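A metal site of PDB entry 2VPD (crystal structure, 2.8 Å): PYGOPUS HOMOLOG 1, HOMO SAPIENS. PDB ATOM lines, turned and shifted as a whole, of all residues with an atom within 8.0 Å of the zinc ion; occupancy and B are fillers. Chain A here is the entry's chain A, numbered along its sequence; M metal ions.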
ATOM      1  N   LEU A  27      13.794  15.347 -22.515  1.00  0.00           N
ATOM      2  CA  LEU A  27      14.423  15.851 -23.718  1.00  0.00           C
ATOM      3  C   LEU A  27      14.399  14.787 -24.812  1.00  0.00           C
ATOM      4  O   LEU A  27      14.802  13.644 -24.577  1.00  0.00           O
ATOM      5  CB  LEU A  27      15.869  16.276 -23.412  1.00  0.00           C
ATOM      6  CG  LEU A  27      16.753  16.849 -24.521  1.00  0.00           C
ATOM      7  CD1 LEU A  27      16.293  18.248 -24.949  1.00  0.00           C
ATOM      8  CD2 LEU A  27      18.207  16.869 -24.099  1.00  0.00           C
ATOM      9  N   CYS A  28      13.942  15.166 -25.994  1.00  0.00           N
ATOM     10  CA  CYS A  28      14.054  14.285 -27.142  1.00  0.00           C
ATOM     11  C   CYS A  28      15.499  14.255 -27.631  1.00  0.00           C
ATOM     12  O   CYS A  28      16.025  15.263 -28.109  1.00  0.00           O
ATOM     13  CB  CYS A  28      13.144  14.711 -28.291  1.00  0.00           C
ATOM     14  SG  CYS A  28      13.445  13.693 -29.761  1.00  0.00           S
ATOM     15  N   GLU A  29      16.121  13.094 -27.498  1.00  0.00           N
ATOM     16  CA  GLU A  29      17.491  12.890 -27.952  1.00  0.00           C
ATOM     17  C   GLU A  29      17.494  12.025 -29.213  1.00  0.00           C
ATOM     18  O   GLU A  29      18.548  11.574 -29.681  1.00  0.00           O
ATOM     19  CB  GLU A  29      18.340  12.259 -26.841  1.00  0.00           C
ATOM     20  CG  GLU A  29      18.265  13.011 -25.525  1.00  0.00           C
ATOM     21  CD  GLU A  29      19.080  12.376 -24.432  1.00  0.00           C
ATOM     22  OE1 GLU A  29      20.321  12.327 -24.577  1.00  0.00           O
ATOM     23  OE2 GLU A  29      18.507  11.922 -23.423  1.00  0.00           O
ATOM     24  N   ALA A  30      16.310  11.801 -29.762  1.00  0.00           N
ATOM     25  CA  ALA A  30      16.183  11.106 -31.042  1.00  0.00           C
ATOM     26  C   ALA A  30      16.615  12.062 -32.154  1.00  0.00           C
ATOM     27  O   ALA A  30      17.310  11.664 -33.077  1.00  0.00           O
ATOM     28  CB  ALA A  30      14.759  10.651 -31.269  1.00  0.00           C
ATOM     29  N   SER A  31      16.197  13.317 -32.031  1.00  0.00           N
ATOM     30  CA  SER A  31      16.533  14.342 -33.017  1.00  0.00           C
ATOM     31  C   SER A  31      16.118  15.742 -32.563  1.00  0.00           C
ATOM     32  O   SER A  31      16.951  16.503 -32.071  1.00  0.00           O
ATOM     33  CB  SER A  31      15.906  14.009 -34.385  1.00  0.00           C
ATOM     34  OG  SER A  31      16.548  14.707 -35.441  1.00  0.00           O
ATOM     35  N   CYS A  32      14.825  16.048 -32.715  1.00  0.00           N
ATOM     36  CA  CYS A  32      14.330  17.421 -32.616  1.00  0.00           C
ATOM     37  C   CYS A  32      14.867  18.236 -31.436  1.00  0.00           C
ATOM     38  O   CYS A  32      14.766  19.480 -31.439  1.00  0.00           O
ATOM     39  CB  CYS A  32      12.794  17.437 -32.624  1.00  0.00           C
ATOM     40  SG  CYS A  32      12.046  17.169 -31.014  1.00  0.00           S
ATOM     41  N   GLN A  33      15.419  17.553 -30.432  1.00  0.00           N
ATOM     42  CA  GLN A  33      16.119  18.189 -29.297  1.00  0.00           C
ATOM     43  C   GLN A  33      15.248  19.082 -28.407  1.00  0.00           C
ATOM     44  O   GLN A  33      15.779  19.839 -27.593  1.00  0.00           O
ATOM     45  CB  GLN A  33      17.356  18.951 -29.789  1.00  0.00           C
ATOM     46  CG  GLN A  33      18.606  18.090 -29.944  1.00  0.00           C
ATOM     47  CD  GLN A  33      19.168  17.580 -28.611  1.00  0.00           C
ATOM     48  OE1 GLN A  33      19.632  16.437 -28.518  1.00  0.00           O
ATOM     49  NE2 GLN A  33      19.122  18.423 -27.587  1.00  0.00           N
ATOM     50  N   LYS A  34      13.934  19.004 -28.565  1.00  0.00           N
ATOM     51  CA  LYS A  34      13.023  19.808 -27.765  1.00  0.00           C
ATOM     52  C   LYS A  34      12.789  19.199 -26.388  1.00  0.00           C
ATOM     53  O   LYS A  34      12.928  17.986 -26.196  1.00  0.00           O
ATOM     54  CB  LYS A  34      11.680  19.972 -28.469  1.00  0.00           C
ATOM     55  CG  LYS A  34      11.750  20.702 -29.790  1.00  0.00           C
ATOM     56  CD  LYS A  34      10.395  20.686 -30.488  1.00  0.00           C
ATOM     57  CE  LYS A  34      10.210  21.942 -31.315  1.00  0.00           C
ATOM     58  NZ  LYS A  34       9.039  21.835 -32.229  1.00  0.00           N
ATOM     59  N   TRP A  35      12.451  20.053 -25.421  1.00  0.00           N
ATOM     60  CA  TRP A  35      11.969  19.620 -24.114  1.00  0.00           C
ATOM     61  C   TRP A  35      10.445  19.503 -24.141  1.00  0.00           C
ATOM     62  O   TRP A  35       9.765  20.232 -24.873  1.00  0.00           O
ATOM     63  CB  TRP A  35      12.402  20.591 -23.014  1.00  0.00           C
ATOM     64  CG  TRP A  35      13.871  20.494 -22.703  1.00  0.00           C
ATOM     65  CD1 TRP A  35      14.885  21.143 -23.342  1.00  0.00           C
ATOM     66  CD2 TRP A  35      14.485  19.701 -21.673  1.00  0.00           C
ATOM     67  NE1 TRP A  35      16.092  20.804 -22.784  1.00  0.00           N
ATOM     68  CE2 TRP A  35      15.875  19.928 -21.756  1.00  0.00           C
ATOM     69  CE3 TRP A  35      13.997  18.832 -20.693  1.00  0.00           C
ATOM     70  CZ2 TRP A  35      16.794  19.303 -20.879  1.00  0.00           C
ATOM     71  CZ3 TRP A  35      14.903  18.215 -19.829  1.00  0.00           C
ATOM     72  CH2 TRP A  35      16.290  18.447 -19.936  1.00  0.00           C
ATOM     73  N   PHE A  36       9.920  18.555 -23.351  1.00  0.00           N
ATOM     74  CA  PHE A  36       8.473  18.319 -23.266  1.00  0.00           C
ATOM     75  C   PHE A  36       8.097  18.044 -21.814  1.00  0.00           C
ATOM     76  O   PHE A  36       8.907  17.518 -21.060  1.00  0.00           O
ATOM     77  CB  PHE A  36       8.096  17.083 -24.092  1.00  0.00           C
ATOM     78  CG  PHE A  36       8.502  17.146 -25.538  1.00  0.00           C
ATOM     79  CD1 PHE A  36       7.553  17.412 -26.527  1.00  0.00           C
ATOM     80  CD2 PHE A  36       9.817  16.907 -25.920  1.00  0.00           C
ATOM     81  CE1 PHE A  36       7.913  17.455 -27.870  1.00  0.00           C
ATOM     82  CE2 PHE A  36      10.191  16.950 -27.260  1.00  0.00           C
ATOM     83  CZ  PHE A  36       9.231  17.228 -28.234  1.00  0.00           C
ATOM     84  N   TRP A  59      15.166   8.890 -24.806  1.00  0.00           N
ATOM     85  CA  TRP A  59      13.785   9.011 -25.254  1.00  0.00           C
ATOM     86  C   TRP A  59      13.682   9.702 -26.606  1.00  0.00           C
ATOM     87  O   TRP A  59      14.495  10.562 -26.943  1.00  0.00           O
ATOM     88  CB  TRP A  59      12.962   9.780 -24.216  1.00  0.00           C
ATOM     89  CG  TRP A  59      11.562  10.023 -24.647  1.00  0.00           C
ATOM     90  CD1 TRP A  59      10.563   9.086 -24.791  1.00  0.00           C
ATOM     91  CD2 TRP A  59      10.979  11.271 -25.012  1.00  0.00           C
ATOM     92  NE1 TRP A  59       9.415   9.678 -25.223  1.00  0.00           N
ATOM     93  CE2 TRP A  59       9.637  11.028 -25.360  1.00  0.00           C
ATOM     94  CE3 TRP A  59      11.463  12.585 -25.080  1.00  0.00           C
ATOM     95  CZ2 TRP A  59       8.773  12.046 -25.773  1.00  0.00           C
ATOM     96  CZ3 TRP A  59      10.597  13.595 -25.482  1.00  0.00           C
ATOM     97  CH2 TRP A  59       9.269  13.312 -25.823  1.00  0.00           C
ATOM     98  N   GLY A  60      12.670   9.331 -27.380  1.00  0.00           N
ATOM     99  CA  GLY A  60      12.354  10.036 -28.624  1.00  0.00           C
ATOM    100  C   GLY A  60      10.883  10.370 -28.748  1.00  0.00           C
ATOM    101  O   GLY A  60      10.027   9.496 -28.572  1.00  0.00           O
ATOM    102  N   CYS A  61      10.584  11.627 -29.050  1.00  0.00           N
ATOM    103  CA  CYS A  61       9.193  12.042 -29.271  1.00  0.00           C
ATOM    104  C   CYS A  61       8.575  11.311 -30.445  1.00  0.00           C
ATOM    105  O   CYS A  61       9.258  10.607 -31.190  1.00  0.00           O
ATOM    106  CB  CYS A  61       9.086  13.558 -29.428  1.00  0.00           C
ATOM    107  SG  CYS A  61       9.663  14.214 -31.006  1.00  0.00           S
ATOM    108  N   ASP A  62       7.272  11.461 -30.609  1.00  0.00           N
ATOM    109  CA  ASP A  62       6.525  10.616 -31.533  1.00  0.00           C
ATOM    110  C   ASP A  62       6.730  10.952 -33.003  1.00  0.00           C
ATOM    111  O   ASP A  62       6.830  10.042 -33.837  1.00  0.00           O
ATOM    112  CB  ASP A  62       5.057  10.583 -31.149  1.00  0.00           C
ATOM    113  CG  ASP A  62       4.845   9.901 -29.805  1.00  0.00           C
ATOM    114  OD1 ASP A  62       5.753   9.177 -29.343  1.00  0.00           O
ATOM    115  OD2 ASP A  62       3.766  10.109 -29.212  1.00  0.00           O
ATOM    116  N   THR A  63       6.807  12.242 -33.325  1.00  0.00           N
ATOM    117  CA  THR A  63       7.134  12.652 -34.684  1.00  0.00           C
ATOM    118  C   THR A  63       8.533  12.166 -35.068  1.00  0.00           C
ATOM    119  O   THR A  63       8.709  11.547 -36.117  1.00  0.00           O
ATOM    120  CB  THR A  63       6.984  14.185 -34.925  1.00  0.00           C
ATOM    121  OG1 THR A  63       6.999  14.878 -33.664  1.00  0.00           O
ATOM    122  CG2 THR A  63       5.656  14.488 -35.646  1.00  0.00           C
ATOM    123  N   CYS A  64       9.507  12.392 -34.187  1.00  0.00           N
ATOM    124  CA  CYS A  64      10.879  11.914 -34.382  1.00  0.00           C
ATOM    125  C   CYS A  64      10.988  10.409 -34.599  1.00  0.00           C
ATOM    126  O   CYS A  64      11.872   9.958 -35.326  1.00  0.00           O
ATOM    127  CB  CYS A  64      11.770  12.329 -33.212  1.00  0.00           C
ATOM    128  SG  CYS A  64      12.478  13.984 -33.363  1.00  0.00           S
ATOM    129  N   MET A  65      10.115   9.628 -33.973  1.00  0.00           N
ATOM    130  CA  MET A  65      10.154   8.161 -34.120  1.00  0.00           C
ATOM    131  C   MET A  65       9.478   7.675 -35.406  1.00  0.00           C
ATOM    132  O   MET A  65       9.868   6.639 -35.957  1.00  0.00           O
ATOM    133  CB  MET A  65       9.520   7.465 -32.910  1.00  0.00           C
ATOM    134  CG  MET A  65      10.212   7.718 -31.574  1.00  0.00           C
ATOM    135  SD  MET A  65      11.918   7.181 -31.500  1.00  0.00           S
ATOM    136  CE  MET A  65      11.759   5.418 -31.313  1.00  0.00           C
HETATM  137 ZN    ZN M   1      11.952  14.785 -31.210  1.00  0.00          ZN
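The side-chain sulfur (SG) of Cys 28 lies close to the backbone NH (N) of Ser 31, 3.6 Å away.
The backbone carbonyl oxygen (O) of Cys 28 sits close to the backbone NH (N) of Gln 33 (3.3 Å).
The side-chain sulfur (SG) of Cys 28 lies close to the backbone NH (N) of Ala 30, at 3.4 Å.
The backbone carbonyl oxygen (O) of Lys 34 is in hydrogen-bond range of the backbone NH (N) of Cys 28 (3.0 Å).
The side-chain sulfur of Cys 32 lies close to the backbone NH of Lys 34 (3.6 Å).
Of the 17 residues printed, 4 come within 4 Å of the zinc ion.
The zinc ion is bound by the side-chain sulfur (SG) of Cys 28 (2.3 Å), the side-chain sulfur (SG) of Cys 64 (2.4 Å), the side-chain sulfur (SG) of Cys 61 (2.4 Å) and the side-chain sulfur (SG) of Cys 32 (2.4 Å).
The zinc ion has four donor atoms within binding distance.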
